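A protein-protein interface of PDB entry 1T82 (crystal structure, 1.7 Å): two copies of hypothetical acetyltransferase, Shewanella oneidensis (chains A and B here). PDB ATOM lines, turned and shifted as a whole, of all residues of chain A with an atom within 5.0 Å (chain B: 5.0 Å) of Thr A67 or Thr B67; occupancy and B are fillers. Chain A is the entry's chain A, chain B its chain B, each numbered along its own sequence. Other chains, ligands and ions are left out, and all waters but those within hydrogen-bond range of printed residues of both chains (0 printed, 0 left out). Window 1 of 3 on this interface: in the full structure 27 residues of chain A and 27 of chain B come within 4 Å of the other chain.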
ATOM      1  N   VAL A  28      -8.064  19.580  -9.418  1.00  0.00           N
ATOM      2  CA  VAL A  28      -6.610  19.670  -9.372  1.00  0.00           C
ATOM      3  C   VAL A  28      -6.102  19.970  -7.964  1.00  0.00           C
ATOM      4  O   VAL A  28      -5.065  19.443  -7.554  1.00  0.00           O
ATOM      5  CB  VAL A  28      -6.085  20.756 -10.354  1.00  0.00           C
ATOM      6  CG1 VAL A  28      -4.644  21.132 -10.010  1.00  0.00           C
ATOM      7  CG2 VAL A  28      -6.146  20.231 -11.772  1.00  0.00           C
ATOM      8  N   MET A  32      -3.415  17.617  -5.957  1.00  0.00           N
ATOM      9  CA  MET A  32      -2.174  18.189  -5.424  1.00  0.00           C
ATOM     10  C   MET A  32      -2.171  18.190  -3.894  1.00  0.00           C
ATOM     11  O   MET A  32      -1.161  18.509  -3.266  1.00  0.00           O
ATOM     12  CB  MET A  32      -1.980  19.623  -5.927  1.00  0.00           C
ATOM     13  CG  MET A  32      -1.783  19.759  -7.426  1.00  0.00           C
ATOM     14  SD  MET A  32      -1.525  21.620  -7.888  1.00  0.00           S
ATOM     15  CE  MET A  32      -0.878  21.424  -9.702  1.00  0.00           C
ATOM     16  N   ILE A  34      -3.595  20.193  -1.716  1.00  0.00           N
ATOM     17  CA  ILE A  34      -3.342  21.519  -1.169  1.00  0.00           C
ATOM     18  C   ILE A  34      -4.300  21.780  -0.011  1.00  0.00           C
ATOM     19  O   ILE A  34      -5.507  21.580  -0.137  1.00  0.00           O
ATOM     20  CB  ILE A  34      -3.534  22.597  -2.266  1.00  0.00           C
ATOM     21  CG1 ILE A  34      -2.510  22.366  -3.383  1.00  0.00           C
ATOM     22  CG2 ILE A  34      -3.388  23.997  -1.666  1.00  0.00           C
ATOM     23  CD1 ILE A  34      -2.652  23.298  -4.586  1.00  0.00           C
ATOM     24  N   PHE A  61       7.200  20.517  -8.675  1.00  0.00           N
ATOM     25  CA  PHE A  61       6.884  20.917 -10.031  1.00  0.00           C
ATOM     26  C   PHE A  61       6.463  22.387 -10.099  1.00  0.00           C
ATOM     27  O   PHE A  61       5.692  22.857  -9.266  1.00  0.00           O
ATOM     28  CB  PHE A  61       5.771  20.004 -10.551  1.00  0.00           C
ATOM     29  CG  PHE A  61       5.207  20.421 -11.866  1.00  0.00           C
ATOM     30  CD1 PHE A  61       6.047  20.735 -12.931  1.00  0.00           C
ATOM     31  CD2 PHE A  61       3.831  20.500 -12.044  1.00  0.00           C
ATOM     32  CE1 PHE A  61       5.518  21.126 -14.153  1.00  0.00           C
ATOM     33  CE2 PHE A  61       3.294  20.891 -13.267  1.00  0.00           C
ATOM     34  CZ  PHE A  61       4.138  21.204 -14.322  1.00  0.00           C
ATOM     35  N   GLY A  63       4.415  23.938 -11.904  1.00  0.00           N
ATOM     36  CA  GLY A  63       2.982  24.142 -11.982  1.00  0.00           C
ATOM     37  C   GLY A  63       2.314  24.008 -10.632  1.00  0.00           C
ATOM     38  O   GLY A  63       1.353  24.715 -10.332  1.00  0.00           O
ATOM     39  N   SER A  64       2.816  23.095  -9.808  1.00  0.00           N
ATOM     40  CA  SER A  64       2.244  22.906  -8.483  1.00  0.00           C
ATOM     41  C   SER A  64       2.597  24.113  -7.628  1.00  0.00           C
ATOM     42  O   SER A  64       1.756  24.616  -6.886  1.00  0.00           O
ATOM     43  CB  SER A  64       2.785  21.625  -7.843  1.00  0.00           C
ATOM     44  OG  SER A  64       2.326  20.488  -8.561  1.00  0.00           O
ATOM     45  N   ILE A  65       3.839  24.577  -7.742  1.00  0.00           N
ATOM     46  CA  ILE A  65       4.285  25.743  -6.987  1.00  0.00           C
ATOM     47  C   ILE A  65       3.356  26.914  -7.305  1.00  0.00           C
ATOM     48  O   ILE A  65       2.818  27.551  -6.401  1.00  0.00           O
ATOM     49  CB  ILE A  65       5.753  26.099  -7.339  1.00  0.00           C
ATOM     50  CG1 ILE A  65       6.681  25.045  -6.724  1.00  0.00           C
ATOM     51  CG2 ILE A  65       6.098  27.511  -6.852  1.00  0.00           C
ATOM     52  CD1 ILE A  65       8.154  25.236  -7.034  1.00  0.00           C
ATOM     53  N   TYR A  66       3.148  27.180  -8.593  1.00  0.00           N
ATOM     54  CA  TYR A  66       2.268  28.271  -9.002  1.00  0.00           C
ATOM     55  C   TYR A  66       0.857  28.078  -8.475  1.00  0.00           C
ATOM     56  O   TYR A  66       0.250  29.006  -7.941  1.00  0.00           O
ATOM     57  CB  TYR A  66       2.177  28.364 -10.524  1.00  0.00           C
ATOM     58  CG  TYR A  66       1.237  29.458 -11.001  1.00  0.00           C
ATOM     59  CD1 TYR A  66       1.692  30.761 -11.170  1.00  0.00           C
ATOM     60  CD2 TYR A  66      -0.110  29.188 -11.270  1.00  0.00           C
ATOM     61  CE1 TYR A  66       0.838  31.775 -11.602  1.00  0.00           C
ATOM     62  CE2 TYR A  66      -0.977  30.201 -11.701  1.00  0.00           C
ATOM     63  CZ  TYR A  66      -0.486  31.493 -11.865  1.00  0.00           C
ATOM     64  OH  TYR A  66      -1.321  32.499 -12.304  1.00  0.00           O
ATOM     65  N   THR A  67       0.330  26.868  -8.630  1.00  0.00           N
ATOM     66  CA  THR A  67      -1.031  26.592  -8.206  1.00  0.00           C
ATOM     67  C   THR A  67      -1.247  26.757  -6.711  1.00  0.00           C
ATOM     68  O   THR A  67      -2.263  27.309  -6.292  1.00  0.00           O
ATOM     69  CB  THR A  67      -1.473  25.188  -8.652  1.00  0.00           C
ATOM     70  OG1 THR A  67      -1.512  25.140 -10.088  1.00  0.00           O
ATOM     71  CG2 THR A  67      -2.864  24.867  -8.116  1.00  0.00           C
ATOM     72  N   ILE A  68      -0.301  26.294  -5.899  1.00  0.00           N
ATOM     73  CA  ILE A  68      -0.468  26.437  -4.460  1.00  0.00           C
ATOM     74  C   ILE A  68      -0.441  27.915  -4.071  1.00  0.00           C
ATOM     75  O   ILE A  68      -1.217  28.349  -3.223  1.00  0.00           O
ATOM     76  CB  ILE A  68       0.608  25.634  -3.675  1.00  0.00           C
ATOM     77  CG1 ILE A  68       0.319  25.698  -2.173  1.00  0.00           C
ATOM     78  CG2 ILE A  68       1.989  26.161  -3.983  1.00  0.00           C
ATOM     79  CD1 ILE A  68       1.166  24.729  -1.362  1.00  0.00           C
ATOM     80  N   MET A  69       0.422  28.698  -4.713  1.00  0.00           N
ATOM     81  CA  MET A  69       0.496  30.120  -4.400  1.00  0.00           C
ATOM     82  C   MET A  69      -0.783  30.841  -4.841  1.00  0.00           C
ATOM     83  O   MET A  69      -1.302  31.695  -4.121  1.00  0.00           O
ATOM     84  CB  MET A  69       1.747  30.725  -5.043  1.00  0.00           C
ATOM     85  CG  MET A  69       3.020  30.044  -4.528  1.00  0.00           C
ATOM     86  SD  MET A  69       4.680  30.609  -5.328  1.00  0.00           S
ATOM     87  CE  MET A  69       5.133  32.026  -4.090  1.00  0.00           C
ATOM     88  N   THR A  70      -1.297  30.476  -6.013  1.00  0.00           N
ATOM     89  CA  THR A  70      -2.530  31.056  -6.534  1.00  0.00           C
ATOM     90  C   THR A  70      -3.680  30.810  -5.559  1.00  0.00           C
ATOM     91  O   THR A  70      -4.458  31.722  -5.255  1.00  0.00           O
ATOM     92  CB  THR A  70      -2.898  30.426  -7.895  1.00  0.00           C
ATOM     93  OG1 THR A  70      -1.954  30.853  -8.883  1.00  0.00           O
ATOM     94  CG2 THR A  70      -4.306  30.821  -8.321  1.00  0.00           C
ATOM     95  N   LEU A  71      -3.794  29.579  -5.067  1.00  0.00           N
ATOM     96  CA  LEU A  71      -4.865  29.253  -4.132  1.00  0.00           C
ATOM     97  C   LEU A  71      -4.652  29.888  -2.761  1.00  0.00           C
ATOM     98  O   LEU A  71      -5.615  30.136  -2.037  1.00  0.00           O
ATOM     99  CB  LEU A  71      -5.029  27.733  -4.008  1.00  0.00           C
ATOM    100  CG  LEU A  71      -5.620  27.072  -5.264  1.00  0.00           C
ATOM    101  CD1 LEU A  71      -5.722  25.566  -5.042  1.00  0.00           C
ATOM    102  CD2 LEU A  71      -7.001  27.655  -5.567  1.00  0.00           C
ATOM    103  N   THR A  72      -3.400  30.157  -2.402  1.00  0.00           N
ATOM    104  CA  THR A  72      -3.131  30.798  -1.120  1.00  0.00           C
ATOM    105  C   THR A  72      -3.661  32.237  -1.208  1.00  0.00           C
ATOM    106  O   THR A  72      -4.308  32.722  -0.277  1.00  0.00           O
ATOM    107  CB  THR A  72      -1.617  30.748  -0.772  1.00  0.00           C
ATOM    108  OG1 THR A  72      -1.226  29.378  -0.583  1.00  0.00           O
ATOM    109  CG2 THR A  72      -1.325  31.511   0.514  1.00  0.00           C
ATOM    110  N   VAL B  28       1.214  15.461 -11.906  1.00  0.00           N
ATOM    111  CA  VAL B  28       0.186  16.472 -12.153  1.00  0.00           C
ATOM    112  C   VAL B  28      -0.164  16.552 -13.639  1.00  0.00           C
ATOM    113  O   VAL B  28      -1.333  16.748 -14.000  1.00  0.00           O
ATOM    114  CB  VAL B  28       0.650  17.877 -11.680  1.00  0.00           C
ATOM    115  CG1 VAL B  28      -0.200  18.968 -12.348  1.00  0.00           C
ATOM    116  CG2 VAL B  28       0.510  17.987 -10.169  1.00  0.00           C
ATOM    117  N   MET B  32      -3.874  16.019 -15.202  1.00  0.00           N
ATOM    118  CA  MET B  32      -4.463  17.058 -16.043  1.00  0.00           C
ATOM    119  C   MET B  32      -4.674  16.601 -17.485  1.00  0.00           C
ATOM    120  O   MET B  32      -5.297  17.309 -18.284  1.00  0.00           O
ATOM    121  CB  MET B  32      -3.576  18.308 -16.032  1.00  0.00           C
ATOM    122  CG  MET B  32      -3.543  19.056 -14.714  1.00  0.00           C
ATOM    123  SD  MET B  32      -2.526  20.685 -14.856  1.00  0.00           S
ATOM    124  CE  MET B  32      -2.831  21.412 -13.096  1.00  0.00           C
ATOM    125  N   ILE B  34      -2.612  16.435 -19.948  1.00  0.00           N
ATOM    126  CA  ILE B  34      -1.985  17.338 -20.906  1.00  0.00           C
ATOM    127  C   ILE B  34      -1.244  16.519 -21.955  1.00  0.00           C
ATOM    128  O   ILE B  34      -0.516  15.581 -21.625  1.00  0.00           O
ATOM    129  CB  ILE B  34      -0.995  18.284 -20.197  1.00  0.00           C
ATOM    130  CG1 ILE B  34      -1.743  19.080 -19.124  1.00  0.00           C
ATOM    131  CG2 ILE B  34      -0.331  19.212 -21.208  1.00  0.00           C
ATOM    132  CD1 ILE B  34      -0.857  19.944 -18.250  1.00  0.00           C
ATOM    133  N   PHE B  61      -9.593  26.077 -14.653  1.00  0.00           N
ATOM    134  CA  PHE B  61      -8.954  26.593 -13.446  1.00  0.00           C
ATOM    135  C   PHE B  61      -7.673  27.357 -13.778  1.00  0.00           C
ATOM    136  O   PHE B  61      -6.857  26.905 -14.585  1.00  0.00           O
ATOM    137  CB  PHE B  61      -8.650  25.411 -12.514  1.00  0.00           C
ATOM    138  CG  PHE B  61      -7.831  25.769 -11.306  1.00  0.00           C
ATOM    139  CD1 PHE B  61      -8.200  26.822 -10.478  1.00  0.00           C
ATOM    140  CD2 PHE B  61      -6.706  25.024 -10.982  1.00  0.00           C
ATOM    141  CE1 PHE B  61      -7.460  27.131  -9.338  1.00  0.00           C
ATOM    142  CE2 PHE B  61      -5.950  25.318  -9.840  1.00  0.00           C
ATOM    143  CZ  PHE B  61      -6.331  26.371  -9.024  1.00  0.00           C
ATOM    144  N   GLY B  63      -4.950  27.683 -12.273  1.00  0.00           N
ATOM    145  CA  GLY B  63      -3.734  26.916 -12.067  1.00  0.00           C
ATOM    146  C   GLY B  63      -3.467  25.953 -13.207  1.00  0.00           C
ATOM    147  O   GLY B  63      -2.321  25.727 -13.582  1.00  0.00           O
ATOM    148  N   SER B  64      -4.526  25.369 -13.757  1.00  0.00           N
ATOM    149  CA  SER B  64      -4.367  24.440 -14.862  1.00  0.00           C
ATOM    150  C   SER B  64      -3.952  25.210 -16.105  1.00  0.00           C
ATOM    151  O   SER B  64      -3.094  24.756 -16.861  1.00  0.00           O
ATOM    152  CB  SER B  64      -5.668  23.674 -15.122  1.00  0.00           C
ATOM    153  OG  SER B  64      -5.975  22.823 -14.028  1.00  0.00           O
ATOM    154  N   ILE B  65      -4.557  26.376 -16.312  1.00  0.00           N
ATOM    155  CA  ILE B  65      -4.217  27.209 -17.458  1.00  0.00           C
ATOM    156  C   ILE B  65      -2.712  27.491 -17.415  1.00  0.00           C
ATOM    157  O   ILE B  65      -2.003  27.271 -18.390  1.00  0.00           O
ATOM    158  CB  ILE B  65      -5.007  28.545 -17.424  1.00  0.00           C
ATOM    159  CG1 ILE B  65      -6.493  28.272 -17.681  1.00  0.00           C
ATOM    160  CG2 ILE B  65      -4.456  29.514 -18.471  1.00  0.00           C
ATOM    161  CD1 ILE B  65      -7.368  29.511 -17.610  1.00  0.00           C
ATOM    162  N   TYR B  66      -2.227  27.963 -16.271  1.00  0.00           N
ATOM    163  CA  TYR B  66      -0.808  28.263 -16.114  1.00  0.00           C
ATOM    164  C   TYR B  66       0.057  27.030 -16.332  1.00  0.00           C
ATOM    165  O   TYR B  66       1.062  27.068 -17.051  1.00  0.00           O
ATOM    166  CB  TYR B  66      -0.515  28.804 -14.716  1.00  0.00           C
ATOM    167  CG  TYR B  66       0.960  29.040 -14.460  1.00  0.00           C
ATOM    168  CD1 TYR B  66       1.555  30.269 -14.757  1.00  0.00           C
ATOM    169  CD2 TYR B  66       1.768  28.025 -13.932  1.00  0.00           C
ATOM    170  CE1 TYR B  66       2.913  30.483 -14.524  1.00  0.00           C
ATOM    171  CE2 TYR B  66       3.128  28.234 -13.705  1.00  0.00           C
ATOM    172  CZ  TYR B  66       3.688  29.462 -14.000  1.00  0.00           C
ATOM    173  OH  TYR B  66       5.022  29.683 -13.751  1.00  0.00           O
ATOM    174  N   THR B  67      -0.328  25.926 -15.705  1.00  0.00           N
ATOM    175  CA  THR B  67       0.457  24.710 -15.825  1.00  0.00           C
ATOM    176  C   THR B  67       0.589  24.213 -17.254  1.00  0.00           C
ATOM    177  O   THR B  67       1.683  23.852 -17.682  1.00  0.00           O
ATOM    178  CB  THR B  67      -0.114  23.588 -14.944  1.00  0.00           C
ATOM    179  OG1 THR B  67      -0.043  23.991 -13.569  1.00  0.00           O
ATOM    180  CG2 THR B  67       0.690  22.307 -15.135  1.00  0.00           C
ATOM    181  N   ILE B  68      -0.508  24.194 -18.007  1.00  0.00           N
ATOM    182  CA  ILE B  68      -0.402  23.722 -19.380  1.00  0.00           C
ATOM    183  C   ILE B  68       0.477  24.662 -20.203  1.00  0.00           C
ATOM    184  O   ILE B  68       1.237  24.214 -21.058  1.00  0.00           O
ATOM    185  CB  ILE B  68      -1.803  23.549 -20.052  1.00  0.00           C
ATOM    186  CG1 ILE B  68      -1.642  23.031 -21.481  1.00  0.00           C
ATOM    187  CG2 ILE B  68      -2.562  24.855 -20.056  1.00  0.00           C
ATOM    188  CD1 ILE B  68      -2.949  22.550 -22.095  1.00  0.00           C
ATOM    189  N   MET B  69       0.397  25.961 -19.935  1.00  0.00           N
ATOM    190  CA  MET B  69       1.214  26.907 -20.681  1.00  0.00           C
ATOM    191  C   MET B  69       2.688  26.751 -20.330  1.00  0.00           C
ATOM    192  O   MET B  69       3.537  26.774 -21.212  1.00  0.00           O
ATOM    193  CB  MET B  69       0.740  28.341 -20.422  1.00  0.00           C
ATOM    194  CG  MET B  69      -0.673  28.563 -20.932  1.00  0.00           C
ATOM    195  SD  MET B  69      -1.416  30.314 -20.625  1.00  0.00           S
ATOM    196  CE  MET B  69      -0.995  31.143 -22.320  1.00  0.00           C
ATOM    197  N   THR B  70       3.001  26.573 -19.052  1.00  0.00           N
ATOM    198  CA  THR B  70       4.396  26.411 -18.693  1.00  0.00           C
ATOM    199  C   THR B  70       4.964  25.097 -19.237  1.00  0.00           C
ATOM    200  O   THR B  70       6.126  25.049 -19.629  1.00  0.00           O
ATOM    201  CB  THR B  70       4.624  26.495 -17.172  1.00  0.00           C
ATOM    202  OG1 THR B  70       6.036  26.535 -16.921  1.00  0.00           O
ATOM    203  CG2 THR B  70       4.015  25.300 -16.467  1.00  0.00           C
ATOM    204  N   LEU B  71       4.158  24.034 -19.277  1.00  0.00           N
ATOM    205  CA  LEU B  71       4.649  22.767 -19.819  1.00  0.00           C
ATOM    206  C   LEU B  71       4.836  22.869 -21.330  1.00  0.00           C
ATOM    207  O   LEU B  71       5.708  22.213 -21.902  1.00  0.00           O
ATOM    208  CB  LEU B  71       3.697  21.610 -19.488  1.00  0.00           C
ATOM    209  CG  LEU B  71       3.802  21.042 -18.070  1.00  0.00           C
ATOM    210  CD1 LEU B  71       2.627  20.119 -17.811  1.00  0.00           C
ATOM    211  CD2 LEU B  71       5.123  20.286 -17.902  1.00  0.00           C
ATOM    212  N   THR B  72       4.025  23.697 -21.982  1.00  0.00           N
ATOM    213  CA  THR B  72       4.146  23.874 -23.422  1.00  0.00           C
ATOM    214  C   THR B  72       5.465  24.588 -23.730  1.00  0.00           C
ATOM    215  O   THR B  72       6.182  24.203 -24.651  1.00  0.00           O
ATOM    216  CB  THR B  72       2.942  24.666 -23.990  1.00  0.00           C
ATOM    217  OG1 THR B  72       1.754  23.879 -23.844  1.00  0.00           O
ATOM    218  CG2 THR B  72       3.142  24.979 -25.470  1.00  0.00           C
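Val A28 touches Met B32 (CG1 to CE, 3.6 Å).
CE of Met A32 touches CG1 of Val B28, 3.7 Å away.
Met A32 touches Met B32.
CZ of Phe A61 touches CG of Leu B71 (3.8 Å).
Val B28 touches Ser A64.
Tyr B66 touches Tyr A66.
CG2 of Thr A67 touches CE2 of Phe B61 (3.6 Å).
Gly B63 touches Thr A67 (CA to OG1, 3.5 Å).
OG1 of Thr A67 touches OG1 of Thr B67, 3.9 Å away.
CD2 of Leu A71 touches CZ of Phe B61 (3.7 Å).
Thr A67 touches three residues of chain B.
Printed residues of chain A within 4 Å of Val B28: Met A32 (3.7 Å) and Ser A64 (3.5 Å).
Of the printed residues of chain A, Phe B61 touches Thr A67 and Leu A71.
Of chain A, only Phe A61 (3.5 Å), Gly A63 (3.4 Å) and Thr A67 (3.9 Å) come within 4 Å of Thr B67.
Thr B70 touches none of the printed residues of chain A.
The nearest residue of chain B that does not touch Thr A67 is Ser B64 (4.8 Å).
OG1 of Thr A67 lies within hydrogen-bond range of O of Gly A63, 2.9 Å away.
The backbone carbonyl oxygen (O) of Tyr A66 is in hydrogen-bond range of the side-chain hydroxyl (OG1) of Thr A70 (3.0 Å).
The side-chain hydroxyl of Thr B67 sits at hydrogen-bond distance from the backbone carbonyl oxygen of Gly B63 (2.9 Å).
Printed residues of chain A that touch a printed residue of chain B: Val A28, Met A32, Phe A61, Gly A63, Ser A64, Tyr A66, Thr A67 and Leu A71.
Hydrophobic or aromatic side chains of chain A within 4 Å of the printed part of chain B: Val A28, Met A32, Phe A61, Tyr A66 and Leu A71.
Val A28 touches Met B32, and with the chains exchanged Met A32 touches Val B28.
Phe A61 touches Thr B67, and with the chains exchanged Thr A67 touches Phe B61.
Phe A61 touches Leu B71, and with the chains exchanged Leu A71 touches Phe B61.
Gly A63 touches Thr B67, and with the chains exchanged Thr A67 touches Gly B63.
14 positions are printed for both chains.
Of the 13 pairs that touch across the chains among the printed residues, 13 have their exchanged pair printed and touching as well.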
